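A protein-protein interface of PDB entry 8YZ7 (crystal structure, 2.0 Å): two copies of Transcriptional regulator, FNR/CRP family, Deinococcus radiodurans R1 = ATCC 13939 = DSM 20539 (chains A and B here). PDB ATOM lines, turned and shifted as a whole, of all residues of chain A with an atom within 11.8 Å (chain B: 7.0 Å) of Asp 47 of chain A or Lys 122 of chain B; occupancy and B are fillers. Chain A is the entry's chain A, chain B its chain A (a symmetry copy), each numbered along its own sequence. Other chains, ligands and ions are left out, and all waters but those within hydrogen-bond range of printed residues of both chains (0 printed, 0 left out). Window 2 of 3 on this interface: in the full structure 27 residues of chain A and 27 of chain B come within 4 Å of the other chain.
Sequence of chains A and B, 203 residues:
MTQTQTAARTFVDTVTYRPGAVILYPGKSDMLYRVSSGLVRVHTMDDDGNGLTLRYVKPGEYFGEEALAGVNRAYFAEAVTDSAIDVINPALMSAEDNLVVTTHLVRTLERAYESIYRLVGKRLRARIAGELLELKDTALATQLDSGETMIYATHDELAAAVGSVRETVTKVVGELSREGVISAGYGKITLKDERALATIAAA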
ATOM      1  N   HIS A  43      -3.601  27.862  -7.547  1.00  0.00           N
ATOM      2  CA  HIS A  43      -3.651  26.421  -7.724  1.00  0.00           C
ATOM      3  C   HIS A  43      -5.068  25.952  -8.018  1.00  0.00           C
ATOM      4  O   HIS A  43      -6.045  26.703  -7.913  1.00  0.00           O
ATOM      5  CB  HIS A  43      -3.135  25.691  -6.493  1.00  0.00           C
ATOM      6  CG  HIS A  43      -3.922  25.983  -5.259  1.00  0.00           C
ATOM      7  ND1 HIS A  43      -4.887  25.128  -4.766  1.00  0.00           N
ATOM      8  CD2 HIS A  43      -3.908  27.053  -4.430  1.00  0.00           C
ATOM      9  CE1 HIS A  43      -5.424  25.654  -3.680  1.00  0.00           C
ATOM     10  NE2 HIS A  43      -4.847  26.822  -3.453  1.00  0.00           N
ATOM     11  N   THR A  44      -5.160  24.669  -8.348  1.00  0.00           N
ATOM     12  CA  THR A  44      -6.442  24.005  -8.564  1.00  0.00           C
ATOM     13  C   THR A  44      -6.309  22.569  -8.074  1.00  0.00           C
ATOM     14  O   THR A  44      -5.288  22.185  -7.496  1.00  0.00           O
ATOM     15  CB  THR A  44      -6.838  24.106 -10.038  1.00  0.00           C
ATOM     16  OG1 THR A  44      -8.138  23.528 -10.231  1.00  0.00           O
ATOM     17  CG2 THR A  44      -5.805  23.399 -10.918  1.00  0.00           C
ATOM     18  N   MET A  45      -7.342  21.770  -8.302  1.00  0.00           N
ATOM     19  CA  MET A  45      -7.330  20.352  -7.974  1.00  0.00           C
ATOM     20  C   MET A  45      -7.518  19.526  -9.239  1.00  0.00           C
ATOM     21  O   MET A  45      -8.278  19.907 -10.132  1.00  0.00           O
ATOM     22  CB  MET A  45      -8.436  19.999  -6.974  1.00  0.00           C
ATOM     23  CG  MET A  45      -8.114  20.373  -5.543  1.00  0.00           C
ATOM     24  SD  MET A  45      -8.348  22.126  -5.176  1.00  0.00           S
ATOM     25  CE  MET A  45      -9.913  22.067  -4.305  1.00  0.00           C
ATOM     26  N   ASP A  46      -6.828  18.385  -9.310  1.00  0.00           N
ATOM     27  CA  ASP A  46      -7.019  17.458 -10.422  1.00  0.00           C
ATOM     28  C   ASP A  46      -8.245  16.579 -10.150  1.00  0.00           C
ATOM     29  O   ASP A  46      -9.016  16.815  -9.213  1.00  0.00           O
ATOM     30  CB  ASP A  46      -5.748  16.637 -10.684  1.00  0.00           C
ATOM     31  CG  ASP A  46      -5.464  15.580  -9.603  1.00  0.00           C
ATOM     32  OD1 ASP A  46      -6.183  15.515  -8.581  1.00  0.00           O
ATOM     33  OD2 ASP A  46      -4.498  14.806  -9.786  1.00  0.00           O
ATOM     34  N   ASP A  47      -8.427  15.536 -10.966  1.00  0.00           N
ATOM     35  CA  ASP A  47      -9.597  14.666 -10.884  1.00  0.00           C
ATOM     36  C   ASP A  47      -9.507  13.634  -9.763  1.00  0.00           C
ATOM     37  O   ASP A  47     -10.486  12.920  -9.524  1.00  0.00           O
ATOM     38  CB  ASP A  47      -9.815  13.943 -12.222  1.00  0.00           C
ATOM     39  CG  ASP A  47      -9.938  14.903 -13.403  1.00  0.00           C
ATOM     40  OD1 ASP A  47      -9.894  16.136 -13.190  1.00  0.00           O
ATOM     41  OD2 ASP A  47     -10.079  14.426 -14.550  1.00  0.00           O
ATOM     42  N   ASP A  48      -8.358  13.512  -9.095  1.00  0.00           N
ATOM     43  CA  ASP A  48      -8.203  12.641  -7.935  1.00  0.00           C
ATOM     44  C   ASP A  48      -8.144  13.426  -6.628  1.00  0.00           C
ATOM     45  O   ASP A  48      -7.828  12.849  -5.583  1.00  0.00           O
ATOM     46  CB  ASP A  48      -6.945  11.777  -8.072  1.00  0.00           C
ATOM     47  CG  ASP A  48      -7.071  10.709  -9.143  1.00  0.00           C
ATOM     48  OD1 ASP A  48      -8.150  10.580  -9.760  1.00  0.00           O
ATOM     49  OD2 ASP A  48      -6.080   9.988  -9.368  1.00  0.00           O
ATOM     50  N   GLY A  49      -8.429  14.725  -6.661  1.00  0.00           N
ATOM     51  CA  GLY A  49      -8.290  15.570  -5.496  1.00  0.00           C
ATOM     52  C   GLY A  49      -6.887  16.075  -5.238  1.00  0.00           C
ATOM     53  O   GLY A  49      -6.700  16.878  -4.314  1.00  0.00           O
ATOM     54  N   ASN A  50      -5.899  15.634  -6.019  1.00  0.00           N
ATOM     55  CA  ASN A  50      -4.521  16.070  -5.821  1.00  0.00           C
ATOM     56  C   ASN A  50      -4.343  17.505  -6.306  1.00  0.00           C
ATOM     57  O   ASN A  50      -4.917  17.918  -7.320  1.00  0.00           O
ATOM     58  CB  ASN A  50      -3.547  15.142  -6.558  1.00  0.00           C
ATOM     59  CG  ASN A  50      -3.792  13.672  -6.260  1.00  0.00           C
ATOM     60  OD1 ASN A  50      -4.699  13.323  -5.505  1.00  0.00           O
ATOM     61  ND2 ASN A  50      -2.988  12.803  -6.869  1.00  0.00           N
ATOM     62  N   GLY A  51      -3.534  18.265  -5.578  1.00  0.00           N
ATOM     63  CA  GLY A  51      -3.367  19.658  -5.900  1.00  0.00           C
ATOM     64  C   GLY A  51      -2.473  19.857  -7.107  1.00  0.00           C
ATOM     65  O   GLY A  51      -1.645  19.017  -7.456  1.00  0.00           O
ATOM     66  N   LEU A  52      -2.648  20.997  -7.758  1.00  0.00           N
ATOM     67  CA  LEU A  52      -1.794  21.385  -8.867  1.00  0.00           C
ATOM     68  C   LEU A  52      -1.523  22.876  -8.767  1.00  0.00           C
ATOM     69  O   LEU A  52      -2.444  23.688  -8.874  1.00  0.00           O
ATOM     70  CB  LEU A  52      -2.432  21.039 -10.205  1.00  0.00           C
ATOM     71  CG  LEU A  52      -1.745  21.772 -11.352  1.00  0.00           C
ATOM     72  CD1 LEU A  52      -0.371  21.175 -11.628  1.00  0.00           C
ATOM     73  CD2 LEU A  52      -2.656  21.698 -12.559  1.00  0.00           C
ATOM     74  N   THR A  53      -0.264  23.233  -8.560  1.00  0.00           N
ATOM     75  CA  THR A  53       0.112  24.633  -8.482  1.00  0.00           C
ATOM     76  C   THR A  53       0.250  25.189  -9.891  1.00  0.00           C
ATOM     77  O   THR A  53       0.990  24.635 -10.715  1.00  0.00           O
ATOM     78  CB  THR A  53       1.426  24.777  -7.715  1.00  0.00           C
ATOM     79  OG1 THR A  53       1.261  24.281  -6.378  1.00  0.00           O
ATOM     80  CG2 THR A  53       1.857  26.239  -7.675  1.00  0.00           C
ATOM     81  N   ALA A  74     -11.299  30.593 -12.160  1.00  0.00           N
ATOM     82  CA  ALA A  74     -11.487  29.159 -12.000  1.00  0.00           C
ATOM     83  C   ALA A  74     -10.462  28.543 -11.059  1.00  0.00           C
ATOM     84  O   ALA A  74     -10.471  27.324 -10.856  1.00  0.00           O
ATOM     85  CB  ALA A  74     -11.435  28.465 -13.362  1.00  0.00           C
ATOM     86  N   PHE A  76      -7.944  28.779  -7.261  1.00  0.00           N
ATOM     87  CA  PHE A  76      -7.799  29.250  -5.894  1.00  0.00           C
ATOM     88  C   PHE A  76      -6.521  30.072  -5.795  1.00  0.00           C
ATOM     89  O   PHE A  76      -5.565  29.847  -6.542  1.00  0.00           O
ATOM     90  CB  PHE A  76      -7.699  28.089  -4.893  1.00  0.00           C
ATOM     91  CG  PHE A  76      -8.897  27.188  -4.856  1.00  0.00           C
ATOM     92  CD1 PHE A  76      -9.159  26.323  -5.902  1.00  0.00           C
ATOM     93  CD2 PHE A  76      -9.740  27.183  -3.752  1.00  0.00           C
ATOM     94  CE1 PHE A  76     -10.254  25.483  -5.869  1.00  0.00           C
ATOM     95  CE2 PHE A  76     -10.837  26.343  -3.711  1.00  0.00           C
ATOM     96  CZ  PHE A  76     -11.092  25.492  -4.776  1.00  0.00           C
ATOM     97  N   LEU A 119       6.642  20.635 -18.530  1.00  0.00           N
ATOM     98  CA  LEU A 119       5.761  19.490 -18.297  1.00  0.00           C
ATOM     99  C   LEU A 119       5.841  18.459 -19.414  1.00  0.00           C
ATOM    100  O   LEU A 119       5.817  17.249 -19.156  1.00  0.00           O
ATOM    101  CB  LEU A 119       4.322  19.961 -18.154  1.00  0.00           C
ATOM    102  CG  LEU A 119       4.012  20.577 -16.807  1.00  0.00           C
ATOM    103  CD1 LEU A 119       2.585  21.067 -16.831  1.00  0.00           C
ATOM    104  CD2 LEU A 119       4.209  19.523 -15.733  1.00  0.00           C
ATOM    105  N   VAL A 120       5.889  18.915 -20.661  1.00  0.00           N
ATOM    106  CA  VAL A 120       5.921  18.000 -21.794  1.00  0.00           C
ATOM    107  C   VAL A 120       7.323  17.473 -22.045  1.00  0.00           C
ATOM    108  O   VAL A 120       7.498  16.294 -22.370  1.00  0.00           O
ATOM    109  CB  VAL A 120       5.366  18.684 -23.062  1.00  0.00           C
ATOM    110  CG1 VAL A 120       5.523  17.766 -24.274  1.00  0.00           C
ATOM    111  CG2 VAL A 120       3.922  19.067 -22.868  1.00  0.00           C
ATOM    112  N   GLY A 163       3.788  18.884 -11.122  1.00  0.00           N
ATOM    113  CA  GLY A 163       2.849  17.987 -11.769  1.00  0.00           C
ATOM    114  C   GLY A 163       3.230  16.529 -11.649  1.00  0.00           C
ATOM    115  O   GLY A 163       3.225  15.783 -12.635  1.00  0.00           O
ATOM    116  N   SER A 164       3.574  16.108 -10.436  1.00  0.00           N
ATOM    117  CA  SER A 164       3.921  14.718 -10.179  1.00  0.00           C
ATOM    118  C   SER A 164       3.133  14.218  -8.974  1.00  0.00           C
ATOM    119  O   SER A 164       2.196  14.882  -8.525  1.00  0.00           O
ATOM    120  CB  SER A 164       5.427  14.572  -9.934  1.00  0.00           C
ATOM    121  OG  SER A 164       5.806  13.204  -9.897  1.00  0.00           O
ATOM    122  N   VAL A 165       3.495  13.050  -8.448  1.00  0.00           N
ATOM    123  CA  VAL A 165       2.879  12.502  -7.250  1.00  0.00           C
ATOM    124  C   VAL A 165       3.965  12.353  -6.200  1.00  0.00           C
ATOM    125  O   VAL A 165       5.147  12.195  -6.517  1.00  0.00           O
ATOM    126  CB  VAL A 165       2.177  11.145  -7.495  1.00  0.00           C
ATOM    127  CG1 VAL A 165       0.997  11.323  -8.432  1.00  0.00           C
ATOM    128  CG2 VAL A 165       3.159  10.125  -8.053  1.00  0.00           C
ATOM    129  N   ILE B 116      -2.275  23.679 -18.810  1.00  0.00           N
ATOM    130  CA  ILE B 116      -1.490  23.029 -17.770  1.00  0.00           C
ATOM    131  C   ILE B 116      -2.328  21.991 -17.039  1.00  0.00           C
ATOM    132  O   ILE B 116      -1.929  20.827 -16.901  1.00  0.00           O
ATOM    133  CB  ILE B 116      -0.939  24.083 -16.792  1.00  0.00           C
ATOM    134  CG1 ILE B 116       0.110  24.945 -17.505  1.00  0.00           C
ATOM    135  CG2 ILE B 116      -0.399  23.417 -15.547  1.00  0.00           C
ATOM    136  CD1 ILE B 116       0.545  26.148 -16.695  1.00  0.00           C
ATOM    137  N   TYR B 117      -3.481  22.409 -16.519  1.00  0.00           N
ATOM    138  CA  TYR B 117      -4.356  21.484 -15.806  1.00  0.00           C
ATOM    139  C   TYR B 117      -4.579  20.210 -16.617  1.00  0.00           C
ATOM    140  O   TYR B 117      -4.445  19.092 -16.100  1.00  0.00           O
ATOM    141  CB  TYR B 117      -5.689  22.176 -15.494  1.00  0.00           C
ATOM    142  CG  TYR B 117      -6.776  21.241 -15.000  1.00  0.00           C
ATOM    143  CD1 TYR B 117      -6.684  20.646 -13.745  1.00  0.00           C
ATOM    144  CD2 TYR B 117      -7.893  20.957 -15.786  1.00  0.00           C
ATOM    145  CE1 TYR B 117      -7.668  19.785 -13.285  1.00  0.00           C
ATOM    146  CE2 TYR B 117      -8.893  20.097 -15.329  1.00  0.00           C
ATOM    147  CZ  TYR B 117      -8.770  19.519 -14.080  1.00  0.00           C
ATOM    148  OH  TYR B 117      -9.748  18.666 -13.616  1.00  0.00           O
ATOM    149  N   ARG B 118      -4.864  20.363 -17.907  1.00  0.00           N
ATOM    150  CA  ARG B 118      -5.219  19.201 -18.718  1.00  0.00           C
ATOM    151  C   ARG B 118      -4.010  18.307 -18.985  1.00  0.00           C
ATOM    152  O   ARG B 118      -4.128  17.077 -18.963  1.00  0.00           O
ATOM    153  CB  ARG B 118      -5.874  19.666 -20.021  1.00  0.00           C
ATOM    154  CG  ARG B 118      -7.199  20.384 -19.746  1.00  0.00           C
ATOM    155  CD  ARG B 118      -7.992  20.655 -21.018  1.00  0.00           C
ATOM    156  NE  ARG B 118      -8.366  19.442 -21.737  1.00  0.00           N
ATOM    157  CZ  ARG B 118      -9.453  18.716 -21.494  1.00  0.00           C
ATOM    158  NH1 ARG B 118     -10.264  18.996 -20.483  1.00  0.00           N
ATOM    159  NH2 ARG B 118      -9.738  17.688 -22.293  1.00  0.00           N
ATOM    160  N   LEU B 119      -2.844  18.904 -19.231  1.00  0.00           N
ATOM    161  CA  LEU B 119      -1.617  18.119 -19.374  1.00  0.00           C
ATOM    162  C   LEU B 119      -1.354  17.229 -18.166  1.00  0.00           C
ATOM    163  O   LEU B 119      -0.909  16.085 -18.314  1.00  0.00           O
ATOM    164  CB  LEU B 119      -0.429  19.043 -19.581  1.00  0.00           C
ATOM    165  CG  LEU B 119      -0.329  19.605 -20.983  1.00  0.00           C
ATOM    166  CD1 LEU B 119       0.839  20.559 -21.026  1.00  0.00           C
ATOM    167  CD2 LEU B 119      -0.132  18.455 -21.955  1.00  0.00           C
ATOM    168  N   VAL B 120      -1.577  17.751 -16.965  1.00  0.00           N
ATOM    169  CA  VAL B 120      -1.308  16.989 -15.754  1.00  0.00           C
ATOM    170  C   VAL B 120      -2.446  16.033 -15.434  1.00  0.00           C
ATOM    171  O   VAL B 120      -2.207  14.901 -15.000  1.00  0.00           O
ATOM    172  CB  VAL B 120      -1.046  17.933 -14.562  1.00  0.00           C
ATOM    173  CG1 VAL B 120      -0.894  17.131 -13.270  1.00  0.00           C
ATOM    174  CG2 VAL B 120       0.180  18.773 -14.813  1.00  0.00           C
ATOM    175  N   GLY B 121      -3.686  16.482 -15.621  1.00  0.00           N
ATOM    176  CA  GLY B 121      -4.844  15.811 -15.063  1.00  0.00           C
ATOM    177  C   GLY B 121      -5.761  15.055 -16.001  1.00  0.00           C
ATOM    178  O   GLY B 121      -6.702  14.409 -15.524  1.00  0.00           O
ATOM    179  N   LYS B 122      -5.533  15.095 -17.320  1.00  0.00           N
ATOM    180  CA  LYS B 122      -6.414  14.422 -18.270  1.00  0.00           C
ATOM    181  C   LYS B 122      -5.664  13.378 -19.090  1.00  0.00           C
ATOM    182  O   LYS B 122      -4.537  13.620 -19.533  1.00  0.00           O
ATOM    183  CB  LYS B 122      -7.070  15.428 -19.220  1.00  0.00           C
ATOM    184  CG  LYS B 122      -7.978  16.430 -18.535  1.00  0.00           C
ATOM    185  CD  LYS B 122      -9.243  15.759 -18.025  1.00  0.00           C
ATOM    186  CE  LYS B 122     -10.174  16.764 -17.370  1.00  0.00           C
ATOM    187  NZ  LYS B 122     -11.414  16.134 -16.842  1.00  0.00           N
ATOM    188  N   ARG B 123      -6.316  12.236 -19.329  1.00  0.00           N
ATOM    189  CA  ARG B 123      -5.795  11.212 -20.222  1.00  0.00           C
ATOM    190  C   ARG B 123      -5.761  11.697 -21.674  1.00  0.00           C
ATOM    191  O   ARG B 123      -6.466  12.625 -22.070  1.00  0.00           O
ATOM    192  CB  ARG B 123      -6.651   9.944 -20.151  1.00  0.00           C
ATOM    193  CG  ARG B 123      -6.779   9.341 -18.773  1.00  0.00           C
ATOM    194  CD  ARG B 123      -5.467   8.736 -18.364  1.00  0.00           C
ATOM    195  NE  ARG B 123      -5.075   7.675 -19.282  1.00  0.00           N
ATOM    196  CZ  ARG B 123      -3.952   6.978 -19.181  1.00  0.00           C
ATOM    197  NH1 ARG B 123      -3.079   7.212 -18.210  1.00  0.00           N
ATOM    198  NH2 ARG B 123      -3.695   6.025 -20.076  1.00  0.00           N
ATOM    199  N   LEU B 124      -4.952  11.015 -22.484  1.00  0.00           N
ATOM    200  CA  LEU B 124      -4.735  11.463 -23.855  1.00  0.00           C
ATOM    201  C   LEU B 124      -6.033  11.500 -24.661  1.00  0.00           C
ATOM    202  O   LEU B 124      -6.232  12.408 -25.473  1.00  0.00           O
ATOM    203  CB  LEU B 124      -3.717  10.571 -24.555  1.00  0.00           C
ATOM    204  CG  LEU B 124      -3.457  10.997 -26.009  1.00  0.00           C
ATOM    205  CD1 LEU B 124      -2.928  12.420 -26.075  1.00  0.00           C
ATOM    206  CD2 LEU B 124      -2.496  10.035 -26.675  1.00  0.00           C
ATOM    207  N   ARG B 125      -6.918  10.515 -24.481  1.00  0.00           N
ATOM    208  CA  ARG B 125      -8.187  10.557 -25.214  1.00  0.00           C
ATOM    209  C   ARG B 125      -8.988  11.805 -24.852  1.00  0.00           C
ATOM    210  O   ARG B 125      -9.619  12.422 -25.718  1.00  0.00           O
ATOM    211  CB  ARG B 125      -9.006   9.296 -24.930  1.00  0.00           C
ATOM    212  CG  ARG B 125      -9.290   9.101 -23.460  1.00  0.00           C
ATOM    213  CD  ARG B 125     -10.013   7.810 -23.173  1.00  0.00           C
ATOM    214  NE  ARG B 125     -11.371   7.820 -23.692  1.00  0.00           N
ATOM    215  CZ  ARG B 125     -11.800   7.033 -24.669  1.00  0.00           C
ATOM    216  NH1 ARG B 125     -10.986   6.194 -25.287  1.00  0.00           N
ATOM    217  NH2 ARG B 125     -13.080   7.084 -25.028  1.00  0.00           N
ATOM    218  N   ALA B 126      -8.952  12.211 -23.581  1.00  0.00           N
ATOM    219  CA  ALA B 126      -9.659  13.424 -23.181  1.00  0.00           C
ATOM    220  C   ALA B 126      -9.028  14.661 -23.799  1.00  0.00           C
ATOM    221  O   ALA B 126      -9.726  15.594 -24.209  1.00  0.00           O
ATOM    222  CB  ALA B 126      -9.677  13.536 -21.657  1.00  0.00           C
ATOM    223  N   ARG B 127      -7.700  14.702 -23.858  1.00  0.00           N
ATOM    224  CA  ARG B 127      -7.047  15.855 -24.465  1.00  0.00           C
ATOM    225  C   ARG B 127      -7.306  15.910 -25.966  1.00  0.00           C
ATOM    226  O   ARG B 127      -7.560  16.983 -26.518  1.00  0.00           O
ATOM    227  CB  ARG B 127      -5.548  15.824 -24.158  1.00  0.00           C
ATOM    228  CG  ARG B 127      -5.259  15.828 -22.632  1.00  0.00           C
ATOM    229  CD  ARG B 127      -3.884  16.385 -22.245  1.00  0.00           C
ATOM    230  NE  ARG B 127      -2.769  15.773 -22.955  1.00  0.00           N
ATOM    231  CZ  ARG B 127      -2.196  14.615 -22.654  1.00  0.00           C
ATOM    232  NH1 ARG B 127      -2.679  13.821 -21.708  1.00  0.00           N
ATOM    233  NH2 ARG B 127      -1.110  14.236 -23.327  1.00  0.00           N
ATOM    234  N   ILE B 200     -16.206  12.873 -23.275  1.00  0.00           N
ATOM    235  CA  ILE B 200     -14.866  12.297 -23.165  1.00  0.00           C
ATOM    236  C   ILE B 200     -13.869  13.364 -22.730  1.00  0.00           C
ATOM    237  O   ILE B 200     -12.994  13.117 -21.885  1.00  0.00           O
ATOM    238  CB  ILE B 200     -14.460  11.655 -24.506  1.00  0.00           C
ATOM    239  CG1 ILE B 200     -15.340  10.442 -24.801  1.00  0.00           C
ATOM    240  CG2 ILE B 200     -12.983  11.279 -24.504  1.00  0.00           C
ATOM    241  CD1 ILE B 200     -15.267   9.994 -26.263  1.00  0.00           C
ATOM    242  N   ALA B 201     -14.001  14.573 -23.280  1.00  0.00           N
ATOM    243  CA  ALA B 201     -13.051  15.640 -22.961  1.00  0.00           C
ATOM    244  C   ALA B 201     -13.134  16.050 -21.494  1.00  0.00           C
ATOM    245  O   ALA B 201     -12.130  16.443 -20.887  1.00  0.00           O
ATOM    246  CB  ALA B 201     -13.292  16.846 -23.862  1.00  0.00           C
ATOM    247  N   ALA B 202     -14.317  15.974 -20.906  1.00  0.00           N
ATOM    248  CA  ALA B 202     -14.470  16.238 -19.483  1.00  0.00           C
ATOM    249  C   ALA B 202     -14.241  14.970 -18.670  1.00  0.00           C
ATOM    250  O   ALA B 202     -14.032  15.039 -17.457  1.00  0.00           O
ATOM    251  CB  ALA B 202     -15.853  16.814 -19.194  1.00  0.00           C
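The side-chain carboxylate of Asp 47 of chain A lies within hydrogen-bond range of the side-chain hydroxyl of Tyr 117 of chain B (2.6 Å). The side-chain carboxylate (OD2) of Asp 47 of chain A is in salt-bridge range of the side-chain amino group (NZ) of Lys 122 of chain B (3.2 Å).
The backbone carbonyl oxygen of Thr 44 of chain A sits at hydrogen-bond distance from the backbone NH of Leu 52 of chain A (2.9 Å). The backbone NH (N) of Asp 48 of chain A is in hydrogen-bond range of the side-chain carboxylate (OD1) of Asp 46 of chain A (3.0 Å). The side-chain carboxylate (OD1) of Asp 46 of chain A is in hydrogen-bond range of the backbone NH (N) of Gly 49 of chain A, 3.1 Å away. OD1 of Asp 46 of chain A is in hydrogen-bond range of N of Asn 50 of chain A (2.6 Å). The backbone carbonyl oxygen of Lys 122 of chain B sits at hydrogen-bond distance from the guanidinium group of Arg 127 of chain B. O of Ala 202 of chain B sits at hydrogen-bond distance from NZ of Lys 122 of chain B (2.9 Å).
O of Met 45 of chain A touches CE1 of Tyr 117 of chain B, 3.2 Å away. CE1 of Tyr 117 of chain B touches CA of Asp 46 of chain A, at 3.7 Å. Gly 121 of chain B touches Asp 47 of chain A (O to OD2, 3.5 Å). CD2 of Leu 52 of chain A touches CA of Tyr 117 of chain B, at 3.7 Å. Val 120 of chain B touches Leu 119 of chain A. CD1 of Leu 119 of chain B touches CG2 of Val 120 of chain A, 3.9 Å away.
Printed residues of chain B within 4 Å of Asp 46 of chain A: Tyr 117. Of the printed residues of chain B, Asp 47 of chain A touches Tyr 117, Gly 121 and Lys 122. Gly 163 of chain A touches none of the printed residues of chain B. Printed residues of chain A within 4 Å of Tyr 117 of chain B: Met 45, Asp 46, Asp 47 and Leu 52. No residue of chain A comes within 4 Å of Arg 118 of chain B. Printed residues of chain A within 4 Å of Leu 119 of chain B: Val 120. Val 120 of chain B touches just one residue of chain A: Leu 119. Lys 122 of chain B touches one residue of chain A. No residue of chain A comes within 4 Å of Arg 123 of chain B. Ala 126 of chain B touches none of the printed residues of chain A. No residue of chain A comes within 4 Å of Ala 201 of chain B. Ala 202 of chain B touches none of the printed residues of chain A. The nearest residue of chain A that does not touch Lys 122 of chain B is Asp 46 of chain A (6.8 Å).
Of the 18 printed residues of chain A, 6 touch a printed residue of chain B. Of the 15 printed residues of chain B, 5 touch a printed residue of chain A. Printed residues of chain B that touch a printed residue of chain A: Tyr 117, Leu 119, Val 120, Gly 121 and Lys 122. Hydrophobic or aromatic side chains of chain B that line the printed part of chain A: Tyr 117, Leu 119 and Val 120. Along chain B the printed residues that touch a printed residue of chain A span positions 117 to 122. Among the printed residues, 8 pairs touch across the chains. Among the printed residues, Asp or Glu carboxylates within 4 Å of a Lys or Arg side-chain nitrogen of the other chain: Asp 47 of chain A with Lys 122 of chain B.
Leu 119 of chain A touches Val 120 of chain B, and with the chains exchanged Val 120 of chain A touches Leu 119 of chain B. 2 positions are printed for both chains. Of the 8 pairs that touch across the chains among the printed residues, 2 have their exchanged pair printed and touching as well.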
